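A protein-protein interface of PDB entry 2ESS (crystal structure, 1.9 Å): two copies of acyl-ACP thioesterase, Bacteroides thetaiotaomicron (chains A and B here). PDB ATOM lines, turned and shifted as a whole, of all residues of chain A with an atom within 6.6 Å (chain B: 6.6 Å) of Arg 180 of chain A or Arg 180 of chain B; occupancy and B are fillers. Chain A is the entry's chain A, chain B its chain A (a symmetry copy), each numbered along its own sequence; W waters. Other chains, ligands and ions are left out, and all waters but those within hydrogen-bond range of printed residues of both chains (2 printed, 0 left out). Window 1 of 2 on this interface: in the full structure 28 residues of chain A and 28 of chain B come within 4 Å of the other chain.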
ATOM      1  N   PHE A  18      26.909  23.527   3.996  1.00  0.00           N
ATOM      2  CA  PHE A  18      26.315  22.268   3.523  1.00  0.00           C
ATOM      3  C   PHE A  18      25.136  22.494   2.608  1.00  0.00           C
ATOM      4  O   PHE A  18      24.491  21.550   2.176  1.00  0.00           O
ATOM      5  CB  PHE A  18      25.969  21.354   4.723  1.00  0.00           C
ATOM      6  CG  PHE A  18      27.176  20.892   5.483  1.00  0.00           C
ATOM      7  CD1 PHE A  18      28.295  20.422   4.814  1.00  0.00           C
ATOM      8  CD2 PHE A  18      27.215  20.944   6.856  1.00  0.00           C
ATOM      9  CE1 PHE A  18      29.412  20.023   5.501  1.00  0.00           C
ATOM     10  CE2 PHE A  18      28.341  20.538   7.533  1.00  0.00           C
ATOM     11  CZ  PHE A  18      29.431  20.080   6.851  1.00  0.00           C
ATOM     12  N   THR A  27      22.326  25.993  -3.387  1.00  0.00           N
ATOM     13  CA  THR A  27      21.809  25.035  -4.329  1.00  0.00           C
ATOM     14  C   THR A  27      20.329  25.403  -4.594  1.00  0.00           C
ATOM     15  O   THR A  27      19.664  26.014  -3.747  1.00  0.00           O
ATOM     16  CB  THR A  27      21.913  23.571  -3.819  1.00  0.00           C
ATOM     17  OG1 THR A  27      21.085  23.416  -2.661  1.00  0.00           O
ATOM     18  CG2 THR A  27      23.387  23.183  -3.469  1.00  0.00           C
ATOM     19  N   VAL A  30      17.980  23.927  -1.948  1.00  0.00           N
ATOM     20  CA  VAL A  30      17.952  24.708  -0.686  1.00  0.00           C
ATOM     21  C   VAL A  30      17.184  25.991  -0.857  1.00  0.00           C
ATOM     22  O   VAL A  30      16.443  26.380   0.060  1.00  0.00           O
ATOM     23  CB  VAL A  30      19.381  24.986  -0.137  1.00  0.00           C
ATOM     24  CG1 VAL A  30      19.337  26.021   0.987  1.00  0.00           C
ATOM     25  CG2 VAL A  30      19.999  23.661   0.330  1.00  0.00           C
ATOM     26  N   SER A 168      15.627   8.851   3.163  1.00  0.00           N
ATOM     27  CA  SER A 168      15.931  10.290   3.141  1.00  0.00           C
ATOM     28  C   SER A 168      15.027  11.125   2.234  1.00  0.00           C
ATOM     29  O   SER A 168      15.025  12.336   2.334  1.00  0.00           O
ATOM     30  CB  SER A 168      17.362  10.492   2.687  1.00  0.00           C
ATOM     31  OG  SER A 168      17.518   9.818   1.441  1.00  0.00           O
ATOM     32  N   ASP A 169      14.303  10.491   1.327  1.00  0.00           N
ATOM     33  CA  ASP A 169      13.401  11.194   0.423  1.00  0.00           C
ATOM     34  C   ASP A 169      12.034  11.518   0.994  1.00  0.00           C
ATOM     35  O   ASP A 169      11.385  12.409   0.472  1.00  0.00           O
ATOM     36  CB  ASP A 169      13.175  10.406  -0.875  1.00  0.00           C
ATOM     37  CG  ASP A 169      14.451  10.248  -1.693  1.00  0.00           C
ATOM     38  OD1 ASP A 169      15.099  11.276  -2.000  1.00  0.00           O
ATOM     39  OD2 ASP A 169      14.808   9.084  -1.998  1.00  0.00           O
ATOM     40  N   ILE A 170      11.628  10.859   2.079  1.00  0.00           N
ATOM     41  CA  ILE A 170      10.217  10.820   2.473  1.00  0.00           C
ATOM     42  C   ILE A 170       9.920  11.780   3.592  1.00  0.00           C
ATOM     43  O   ILE A 170      10.664  11.837   4.568  1.00  0.00           O
ATOM     44  CB  ILE A 170       9.815   9.396   2.882  1.00  0.00           C
ATOM     45  CG1 ILE A 170      10.241   8.391   1.809  1.00  0.00           C
ATOM     46  CG2 ILE A 170       8.293   9.281   3.183  1.00  0.00           C
ATOM     47  CD1 ILE A 170       9.556   8.601   0.436  1.00  0.00           C
ATOM     48  N   VAL A 176       7.594  11.303  -1.248  1.00  0.00           N
ATOM     49  CA  VAL A 176       8.797  11.950  -1.661  1.00  0.00           C
ATOM     50  C   VAL A 176       8.554  13.441  -1.672  1.00  0.00           C
ATOM     51  O   VAL A 176       7.599  13.923  -2.269  1.00  0.00           O
ATOM     52  CB  VAL A 176       9.272  11.449  -3.038  1.00  0.00           C
ATOM     53  CG1 VAL A 176      10.472  12.295  -3.516  1.00  0.00           C
ATOM     54  CG2 VAL A 176       9.635  10.041  -2.926  1.00  0.00           C
ATOM     55  N   ASN A 177       9.405  14.180  -0.978  1.00  0.00           N
ATOM     56  CA  ASN A 177       9.134  15.575  -0.775  1.00  0.00           C
ATOM     57  C   ASN A 177       9.524  16.430  -1.997  1.00  0.00           C
ATOM     58  O   ASN A 177      10.305  16.010  -2.868  1.00  0.00           O
ATOM     59  CB  ASN A 177       9.626  16.042   0.626  1.00  0.00           C
ATOM     60  CG  ASN A 177      11.066  16.481   0.664  1.00  0.00           C
ATOM     61  OD1 ASN A 177      11.525  17.145  -0.228  1.00  0.00           O
ATOM     62  ND2 ASN A 177      11.764  16.181   1.774  1.00  0.00           N
ATOM     63  N   SER A 178       8.888  17.592  -2.077  1.00  0.00           N
ATOM     64  CA  SER A 178       9.051  18.535  -3.171  1.00  0.00           C
ATOM     65  C   SER A 178      10.494  18.864  -3.530  1.00  0.00           C
ATOM     66  O   SER A 178      10.855  18.973  -4.720  1.00  0.00           O
ATOM     67  CB  SER A 178       8.386  19.853  -2.770  1.00  0.00           C
ATOM     68  OG  SER A 178       7.033  19.658  -2.501  1.00  0.00           O
ATOM     69  N   ILE A 179      11.312  19.026  -2.487  1.00  0.00           N
ATOM     70  CA  ILE A 179      12.704  19.423  -2.627  1.00  0.00           C
ATOM     71  C   ILE A 179      13.586  18.274  -3.083  1.00  0.00           C
ATOM     72  O   ILE A 179      14.550  18.480  -3.809  1.00  0.00           O
ATOM     73  CB  ILE A 179      13.234  19.997  -1.283  1.00  0.00           C
ATOM     74  CG1 ILE A 179      12.387  21.187  -0.866  1.00  0.00           C
ATOM     75  CG2 ILE A 179      14.663  20.452  -1.399  1.00  0.00           C
ATOM     76  CD1 ILE A 179      12.159  22.176  -1.968  1.00  0.00           C
ATOM     77  N   ARG A 180      13.274  17.062  -2.647  1.00  0.00           N
ATOM     78  CA  ARG A 180      14.045  15.913  -3.041  1.00  0.00           C
ATOM     79  C   ARG A 180      13.912  15.664  -4.529  1.00  0.00           C
ATOM     80  O   ARG A 180      14.881  15.273  -5.156  1.00  0.00           O
ATOM     81  CB  ARG A 180      13.621  14.678  -2.251  1.00  0.00           C
ATOM     82  CG  ARG A 180      14.033  14.769  -0.784  1.00  0.00           C
ATOM     83  CD  ARG A 180      15.508  14.522  -0.645  1.00  0.00           C
ATOM     84  NE  ARG A 180      16.009  14.983   0.640  1.00  0.00           N
ATOM     85  CZ  ARG A 180      17.266  14.791   1.050  1.00  0.00           C
ATOM     86  NH1 ARG A 180      18.131  14.127   0.285  1.00  0.00           N
ATOM     87  NH2 ARG A 180      17.656  15.245   2.234  1.00  0.00           N
ATOM     88  N   TYR A 181      12.743  15.932  -5.116  1.00  0.00           N
ATOM     89  CA  TYR A 181      12.638  15.837  -6.571  1.00  0.00           C
ATOM     90  C   TYR A 181      13.584  16.793  -7.298  1.00  0.00           C
ATOM     91  O   TYR A 181      14.144  16.429  -8.324  1.00  0.00           O
ATOM     92  CB  TYR A 181      11.237  16.119  -7.047  1.00  0.00           C
ATOM     93  CG  TYR A 181      10.195  15.069  -6.783  1.00  0.00           C
ATOM     94  CD1 TYR A 181      10.242  13.804  -7.403  1.00  0.00           C
ATOM     95  CD2 TYR A 181       9.115  15.348  -5.959  1.00  0.00           C
ATOM     96  CE1 TYR A 181       9.228  12.849  -7.191  1.00  0.00           C
ATOM     97  CE2 TYR A 181       8.105  14.404  -5.746  1.00  0.00           C
ATOM     98  CZ  TYR A 181       8.157  13.165  -6.370  1.00  0.00           C
ATOM     99  OH  TYR A 181       7.105  12.294  -6.123  1.00  0.00           O
ATOM    100  N   ILE A 182      13.689  18.026  -6.801  1.00  0.00           N
ATOM    101  CA  ILE A 182      14.623  19.020  -7.349  1.00  0.00           C
ATOM    102  C   ILE A 182      16.063  18.510  -7.339  1.00  0.00           C
ATOM    103  O   ILE A 182      16.743  18.532  -8.381  1.00  0.00           O
ATOM    104  CB  ILE A 182      14.533  20.362  -6.592  1.00  0.00           C
ATOM    105  CG1 ILE A 182      13.124  20.957  -6.768  1.00  0.00           C
ATOM    106  CG2 ILE A 182      15.593  21.346  -7.101  1.00  0.00           C
ATOM    107  CD1 ILE A 182      12.901  22.309  -6.018  1.00  0.00           C
ATOM    108  N   GLU A 183      16.528  18.046  -6.181  1.00  0.00           N
ATOM    109  CA  GLU A 183      17.869  17.466  -6.068  1.00  0.00           C
ATOM    110  C   GLU A 183      18.119  16.332  -7.055  1.00  0.00           C
ATOM    111  O   GLU A 183      19.158  16.292  -7.707  1.00  0.00           O
ATOM    112  CB  GLU A 183      18.121  16.914  -4.669  1.00  0.00           C
ATOM    113  CG  GLU A 183      18.275  17.989  -3.572  1.00  0.00           C
ATOM    114  CD  GLU A 183      18.582  17.390  -2.163  1.00  0.00           C
ATOM    115  OE1 GLU A 183      18.968  16.179  -2.101  1.00  0.00           O
ATOM    116  OE2 GLU A 183      18.438  18.136  -1.146  1.00  0.00           O
ATOM    117  N   HIS A 184      17.181  15.388  -7.152  1.00  0.00           N
ATOM    118  CA  HIS A 184      17.397  14.262  -8.074  1.00  0.00           C
ATOM    119  C   HIS A 184      17.436  14.704  -9.556  1.00  0.00           C
ATOM    120  O   HIS A 184      18.196  14.183 -10.330  1.00  0.00           O
ATOM    121  CB  HIS A 184      16.362  13.160  -7.839  1.00  0.00           C
ATOM    122  CG  HIS A 184      16.455  12.541  -6.475  1.00  0.00           C
ATOM    123  ND1 HIS A 184      17.628  12.014  -5.975  1.00  0.00           N
ATOM    124  CD2 HIS A 184      15.527  12.386  -5.500  1.00  0.00           C
ATOM    125  CE1 HIS A 184      17.417  11.566  -4.747  1.00  0.00           C
ATOM    126  NE2 HIS A 184      16.149  11.775  -4.440  1.00  0.00           N
ATOM    127  N   ILE A 185      16.615  15.677  -9.934  1.00  0.00           N
ATOM    128  CA  ILE A 185      16.587  16.156 -11.309  1.00  0.00           C
ATOM    129  C   ILE A 185      17.913  16.834 -11.652  1.00  0.00           C
ATOM    130  O   ILE A 185      18.525  16.567 -12.712  1.00  0.00           O
ATOM    131  CB  ILE A 185      15.361  17.101 -11.539  1.00  0.00           C
ATOM    132  CG1 ILE A 185      14.064  16.282 -11.508  1.00  0.00           C
ATOM    133  CG2 ILE A 185      15.461  17.847 -12.874  1.00  0.00           C
ATOM    134  CD1 ILE A 185      12.860  17.110 -11.316  1.00  0.00           C
ATOM    135  N   ASP A 187      20.714  16.341 -10.324  1.00  0.00           N
ATOM    136  CA  ASP A 187      21.800  15.323 -10.445  1.00  0.00           C
ATOM    137  C   ASP A 187      21.900  14.642 -11.799  1.00  0.00           C
ATOM    138  O   ASP A 187      22.852  13.945 -12.028  1.00  0.00           O
ATOM    139  CB  ASP A 187      21.712  14.240  -9.355  1.00  0.00           C
ATOM    140  CG  ASP A 187      22.094  14.772  -7.942  1.00  0.00           C
ATOM    141  OD1 ASP A 187      22.867  15.747  -7.871  1.00  0.00           O
ATOM    142  OD2 ASP A 187      21.632  14.210  -6.912  1.00  0.00           O
ATOM    143  N   PHE B  18      10.684  19.925   5.587  1.00  0.00           N
ATOM    144  CA  PHE B  18      11.581  19.206   4.670  1.00  0.00           C
ATOM    145  C   PHE B  18      12.807  18.668   5.366  1.00  0.00           C
ATOM    146  O   PHE B  18      13.683  18.098   4.733  1.00  0.00           O
ATOM    147  CB  PHE B  18      11.930  20.097   3.454  1.00  0.00           C
ATOM    148  CG  PHE B  18      10.746  20.412   2.590  1.00  0.00           C
ATOM    149  CD1 PHE B  18       9.851  19.416   2.229  1.00  0.00           C
ATOM    150  CD2 PHE B  18      10.502  21.692   2.155  1.00  0.00           C
ATOM    151  CE1 PHE B  18       8.751  19.701   1.462  1.00  0.00           C
ATOM    152  CE2 PHE B  18       9.398  21.963   1.383  1.00  0.00           C
ATOM    153  CZ  PHE B  18       8.530  20.967   1.041  1.00  0.00           C
ATOM    154  N   THR B  27      15.675  14.792  11.096  1.00  0.00           N
ATOM    155  CA  THR B  27      16.503  13.720  10.610  1.00  0.00           C
ATOM    156  C   THR B  27      17.900  13.889  11.253  1.00  0.00           C
ATOM    157  O   THR B  27      18.301  15.002  11.618  1.00  0.00           O
ATOM    158  CB  THR B  27      16.625  13.706   9.061  1.00  0.00           C
ATOM    159  OG1 THR B  27      17.294  14.896   8.631  1.00  0.00           O
ATOM    160  CG2 THR B  27      15.225  13.609   8.370  1.00  0.00           C
ATOM    161  N   VAL B  30      20.099  16.345   9.296  1.00  0.00           N
ATOM    162  CA  VAL B  30      19.790  17.768   9.584  1.00  0.00           C
ATOM    163  C   VAL B  30      20.300  18.173  10.942  1.00  0.00           C
ATOM    164  O   VAL B  30      20.809  19.295  11.087  1.00  0.00           O
ATOM    165  CB  VAL B  30      18.271  18.077   9.448  1.00  0.00           C
ATOM    166  CG1 VAL B  30      17.946  19.457  10.020  1.00  0.00           C
ATOM    167  CG2 VAL B  30      17.874  17.964   7.970  1.00  0.00           C
ATOM    168  N   SER B 168      24.696  16.766  -6.119  1.00  0.00           N
ATOM    169  CA  SER B 168      24.114  17.141  -4.821  1.00  0.00           C
ATOM    170  C   SER B 168      24.950  16.749  -3.604  1.00  0.00           C
ATOM    171  O   SER B 168      24.694  17.226  -2.517  1.00  0.00           O
ATOM    172  CB  SER B 168      22.750  16.496  -4.679  1.00  0.00           C
ATOM    173  OG  SER B 168      22.912  15.096  -4.892  1.00  0.00           O
ATOM    174  N   ASP B 169      25.908  15.853  -3.772  1.00  0.00           N
ATOM    175  CA  ASP B 169      26.769  15.420  -2.678  1.00  0.00           C
ATOM    176  C   ASP B 169      27.948  16.328  -2.383  1.00  0.00           C
ATOM    177  O   ASP B 169      28.471  16.258  -1.284  1.00  0.00           O
ATOM    178  CB  ASP B 169      27.330  14.013  -2.923  1.00  0.00           C
ATOM    179  CG  ASP B 169      26.242  12.948  -2.966  1.00  0.00           C
ATOM    180  OD1 ASP B 169      25.450  12.859  -1.998  1.00  0.00           O
ATOM    181  OD2 ASP B 169      26.174  12.223  -3.989  1.00  0.00           O
ATOM    182  N   ILE B 170      28.320  17.206  -3.314  1.00  0.00           N
ATOM    183  CA  ILE B 170      29.639  17.843  -3.287  1.00  0.00           C
ATOM    184  C   ILE B 170      29.574  19.244  -2.746  1.00  0.00           C
ATOM    185  O   ILE B 170      28.704  20.017  -3.139  1.00  0.00           O
ATOM    186  CB  ILE B 170      30.258  17.851  -4.693  1.00  0.00           C
ATOM    187  CG1 ILE B 170      30.200  16.451  -5.310  1.00  0.00           C
ATOM    188  CG2 ILE B 170      31.714  18.399  -4.688  1.00  0.00           C
ATOM    189  CD1 ILE B 170      31.016  15.384  -4.540  1.00  0.00           C
ATOM    190  N   VAL B 176      32.611  15.078  -1.171  1.00  0.00           N
ATOM    191  CA  VAL B 176      31.373  14.658  -0.598  1.00  0.00           C
ATOM    192  C   VAL B 176      31.310  15.171   0.822  1.00  0.00           C
ATOM    193  O   VAL B 176      32.223  14.963   1.612  1.00  0.00           O
ATOM    194  CB  VAL B 176      31.210  13.128  -0.650  1.00  0.00           C
ATOM    195  CG1 VAL B 176      29.944  12.711   0.131  1.00  0.00           C
ATOM    196  CG2 VAL B 176      31.126  12.711  -2.045  1.00  0.00           C
ATOM    197  N   ASN B 177      30.238  15.877   1.143  1.00  0.00           N
ATOM    198  CA  ASN B 177      30.190  16.562   2.404  1.00  0.00           C
ATOM    199  C   ASN B 177      29.813  15.624   3.566  1.00  0.00           C
ATOM    200  O   ASN B 177      29.265  14.525   3.370  1.00  0.00           O
ATOM    201  CB  ASN B 177      29.421  17.910   2.278  1.00  0.00           C
ATOM    202  CG  ASN B 177      27.931  17.794   2.468  1.00  0.00           C
ATOM    203  OD1 ASN B 177      27.479  17.086   3.328  1.00  0.00           O
ATOM    204  ND2 ASN B 177      27.158  18.587   1.703  1.00  0.00           N
ATOM    205  N   SER B 178      30.207  16.047   4.761  1.00  0.00           N
ATOM    206  CA  SER B 178      30.013  15.300   5.993  1.00  0.00           C
ATOM    207  C   SER B 178      28.600  14.781   6.218  1.00  0.00           C
ATOM    208  O   SER B 178      28.396  13.640   6.683  1.00  0.00           O
ATOM    209  CB  SER B 178      30.335  16.224   7.169  1.00  0.00           C
ATOM    210  OG  SER B 178      31.648  16.685   7.086  1.00  0.00           O
ATOM    211  N   ILE B 179      27.626  15.633   5.889  1.00  0.00           N
ATOM    212  CA  ILE B 179      26.217  15.350   6.108  1.00  0.00           C
ATOM    213  C   ILE B 179      25.659  14.384   5.078  1.00  0.00           C
ATOM    214  O   ILE B 179      24.786  13.583   5.385  1.00  0.00           O
ATOM    215  CB  ILE B 179      25.397  16.670   6.096  1.00  0.00           C
ATOM    216  CG1 ILE B 179      25.918  17.605   7.173  1.00  0.00           C
ATOM    217  CG2 ILE B 179      23.936  16.419   6.356  1.00  0.00           C
ATOM    218  CD1 ILE B 179      26.097  16.944   8.506  1.00  0.00           C
ATOM    219  N   ARG B 180      26.144  14.466   3.846  1.00  0.00           N
ATOM    220  CA  ARG B 180      25.684  13.580   2.811  1.00  0.00           C
ATOM    221  C   ARG B 180      26.074  12.149   3.117  1.00  0.00           C
ATOM    222  O   ARG B 180      25.303  11.249   2.836  1.00  0.00           O
ATOM    223  CB  ARG B 180      26.232  14.005   1.451  1.00  0.00           C
ATOM    224  CG  ARG B 180      25.606  15.311   0.965  1.00  0.00           C
ATOM    225  CD  ARG B 180      24.207  15.064   0.479  1.00  0.00           C
ATOM    226  NE  ARG B 180      23.446  16.299   0.388  1.00  0.00           N
ATOM    227  CZ  ARG B 180      22.209  16.364  -0.112  1.00  0.00           C
ATOM    228  NH1 ARG B 180      21.613  15.270  -0.583  1.00  0.00           N
ATOM    229  NH2 ARG B 180      21.571  17.527  -0.160  1.00  0.00           N
ATOM    230  N   TYR B 181      27.236  11.927   3.736  1.00  0.00           N
ATOM    231  CA  TYR B 181      27.564  10.569   4.170  1.00  0.00           C
ATOM    232  C   TYR B 181      26.557  10.009   5.175  1.00  0.00           C
ATOM    233  O   TYR B 181      26.234   8.830   5.116  1.00  0.00           O
ATOM    234  CB  TYR B 181      28.932  10.501   4.796  1.00  0.00           C
ATOM    235  CG  TYR B 181      30.116  10.621   3.878  1.00  0.00           C
ATOM    236  CD1 TYR B 181      30.414   9.636   2.916  1.00  0.00           C
ATOM    237  CD2 TYR B 181      30.989  11.692   4.003  1.00  0.00           C
ATOM    238  CE1 TYR B 181      31.559   9.734   2.101  1.00  0.00           C
ATOM    239  CE2 TYR B 181      32.129  11.792   3.197  1.00  0.00           C
ATOM    240  CZ  TYR B 181      32.417  10.810   2.260  1.00  0.00           C
ATOM    241  OH  TYR B 181      33.577  10.975   1.515  1.00  0.00           O
ATOM    242  N   ILE B 182      26.136  10.839   6.129  1.00  0.00           N
ATOM    243  CA  ILE B 182      25.108  10.459   7.108  1.00  0.00           C
ATOM    244  C   ILE B 182      23.815  10.016   6.428  1.00  0.00           C
ATOM    245  O   ILE B 182      23.299   8.921   6.715  1.00  0.00           O
ATOM    246  CB  ILE B 182      24.818  11.606   8.101  1.00  0.00           C
ATOM    247  CG1 ILE B 182      26.088  11.916   8.914  1.00  0.00           C
ATOM    248  CG2 ILE B 182      23.664  11.233   9.040  1.00  0.00           C
ATOM    249  CD1 ILE B 182      25.925  13.085   9.936  1.00  0.00           C
ATOM    250  N   GLU B 183      23.293  10.848   5.529  1.00  0.00           N
ATOM    251  CA  GLU B 183      22.094  10.498   4.762  1.00  0.00           C
ATOM    252  C   GLU B 183      22.221   9.173   4.020  1.00  0.00           C
ATOM    253  O   GLU B 183      21.315   8.346   4.063  1.00  0.00           O
ATOM    254  CB  GLU B 183      21.763  11.568   3.727  1.00  0.00           C
ATOM    255  CG  GLU B 183      21.242  12.895   4.319  1.00  0.00           C
ATOM    256  CD  GLU B 183      20.865  13.948   3.229  1.00  0.00           C
ATOM    257  OE1 GLU B 183      20.726  13.543   2.031  1.00  0.00           O
ATOM    258  OE2 GLU B 183      20.709  15.156   3.586  1.00  0.00           O
ATOM    259  N   HIS B 184      23.334   8.972   3.312  1.00  0.00           N
ATOM    260  CA  HIS B 184      23.482   7.717   2.560  1.00  0.00           C
ATOM    261  C   HIS B 184      23.565   6.476   3.480  1.00  0.00           C
ATOM    262  O   HIS B 184      23.044   5.440   3.159  1.00  0.00           O
ATOM    263  CB  HIS B 184      24.674   7.793   1.603  1.00  0.00           C
ATOM    264  CG  HIS B 184      24.515   8.842   0.542  1.00  0.00           C
ATOM    265  ND1 HIS B 184      23.414   8.901  -0.287  1.00  0.00           N
ATOM    266  CD2 HIS B 184      25.307   9.883   0.190  1.00  0.00           C
ATOM    267  CE1 HIS B 184      23.535   9.938  -1.100  1.00  0.00           C
ATOM    268  NE2 HIS B 184      24.678  10.545  -0.835  1.00  0.00           N
ATOM    269  N   ILE B 185      24.218   6.600   4.630  1.00  0.00           N
ATOM    270  CA  ILE B 185      24.343   5.485   5.557  1.00  0.00           C
ATOM    271  C   ILE B 185      22.971   5.114   6.116  1.00  0.00           C
ATOM    272  O   ILE B 185      22.582   3.925   6.152  1.00  0.00           O
ATOM    273  CB  ILE B 185      25.374   5.819   6.687  1.00  0.00           C
ATOM    274  CG1 ILE B 185      26.792   5.849   6.101  1.00  0.00           C
ATOM    275  CG2 ILE B 185      25.316   4.799   7.829  1.00  0.00           C
ATOM    276  CD1 ILE B 185      27.764   6.533   6.971  1.00  0.00           C
ATOM    277  N   ASP B 187      20.167   5.623   4.800  1.00  0.00           N
ATOM    278  CA  ASP B 187      19.337   4.969   3.745  1.00  0.00           C
ATOM    279  C   ASP B 187      19.570   3.478   3.572  1.00  0.00           C
ATOM    280  O   ASP B 187      18.821   2.853   2.871  1.00  0.00           O
ATOM    281  CB  ASP B 187      19.487   5.653   2.374  1.00  0.00           C
ATOM    282  CG  ASP B 187      18.809   7.054   2.320  1.00  0.00           C
ATOM    283  OD1 ASP B 187      17.853   7.274   3.089  1.00  0.00           O
ATOM    284  OD2 ASP B 187      19.224   7.923   1.506  1.00  0.00           O
HETATM  285  O   HOH W   1      24.283  18.756   2.018  1.00  0.00           O
HETATM  286  O   HOH W   2      14.471  17.106   2.229  1.00  0.00           O
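The side-chain hydroxyl (OG) of Ser 168 of chain B lies within hydrogen-bond range of the side-chain carboxylate (OD2) of Asp 187 of chain A (2.6 Å).
The guanidinium group (NH1) of Arg 180 of chain A lies within salt-bridge range of the side-chain carboxylate (OE1) of Glu 183 of chain B, at 3.2 Å.
OD2 of Asp 187 of chain B is in hydrogen-bond range of OG of Ser 168 of chain A.
The side-chain carboxylate (OE1) of Glu 183 of chain A lies within salt-bridge range of the guanidinium group (NH1) of Arg 180 of chain B (3.2 Å).
The backbone NH (N) of Ile 179 of chain B sits at hydrogen-bond distance from the side-chain amide oxygen (OD1) of Asn 177 of chain B (2.9 Å).
The backbone carbonyl oxygen (O) of Asp 169 of chain B lies within hydrogen-bond range of the backbone NH (N) of Asn 177 of chain B (3.0 Å).
O of Ser 168 of chain A lies within hydrogen-bond range of NE of Arg 180 of chain A (3.3 Å).
N of Arg 180 of chain B is in hydrogen-bond range of OD1 of Asn 177 of chain B, 3.0 Å away.
The backbone carbonyl oxygen (O) of Ser 168 of chain B lies within hydrogen-bond range of the guanidinium group (NE) of Arg 180 of chain B (3.3 Å).
NH1 of Arg 180 of chain B lies within salt-bridge range of OE1 of Glu 183 of chain B, at 3.3 Å.
Among the printed residues, pairs that only touch across the chains: Phe 18 of chain A with Asn 177 of chain B, Phe 18 of chain A with Ser 178 of chain B, Phe 18 of chain A with Ile 179 of chain B, Asn 177 of chain A with Phe 18 of chain B, Ser 178 of chain A with Phe 18 of chain B, Ile 179 of chain A with Phe 18 of chain B and Arg 180 of chain A with Arg 180 of chain B.
Of the printed residues of chain B, Ser 168 of chain A touches Asp 187.
Val 176 of chain A touches none of the printed residues of chain B.
Arg 180 of chain A touches just these residues of chain B: Arg 180 and Glu 183.
Of the printed residues of chain A, Phe 18 of chain B touches Asn 177, Ser 178 and Ile 179.
Of the printed residues of chain A, Ser 168 of chain B touches Asp 187 (2.6 Å).
Val 176 of chain B touches none of the printed residues of chain A.
Printed residues of chain A within 4 Å of Arg 180 of chain B: Arg 180 and Glu 183.
Printed residues of chain B that touch a printed residue of chain A: Phe 18, Ser 168, Asn 177, Ser 178, Ile 179, Arg 180, Glu 183 and Asp 187.
Hydrophobic or aromatic side chains of chain A that line the printed part of chain B: Phe 18 and Ile 179.
Among the printed residues, 11 pairs touch across the chains.
Among the printed residues, Asp or Glu carboxylates within 4 Å of a Lys or Arg side-chain nitrogen of the other chain: Arg 180 of chain A with Glu 183 of chain B and Glu 183 of chain A with Arg 180 of chain B.
Phe 18 of chain A touches Ser 178 of chain B, and with the chains exchanged Ser 178 of chain A touches Phe 18 of chain B.
Phe 18 of chain A touches Ile 179 of chain B, and with the chains exchanged Ile 179 of chain A touches Phe 18 of chain B.
Ser 168 of chain A touches Asp 187 of chain B, and with the chains exchanged Asp 187 of chain A touches Ser 168 of chain B.
Arg 180 of chain B touches its own counterpart, Arg 180 of chain A.
Positions printed for both chains: 18, 27, 30, 168, 169, 170, 176, 177, 178, 179, 180, 181, 182, 183, 184, 185 and 187.
Of the 11 pairs that touch across the chains among the printed residues, 11 have their exchanged pair printed and touching as well.
Water W1 lies within hydrogen-bond range of O of Phe 18 of chain A, ND2 of Asn 177 of chain B and NE of Arg 180 of chain B.
Water W2 lies within hydrogen-bond range of the backbone carbonyl oxygen (O) of Phe 18 of chain B (2.8 Å), the side-chain amide nitrogen (ND2) of Asn 177 of chain A (2.9 Å) and the guanidinium group (NE) of Arg 180 of chain A (3.1 Å).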
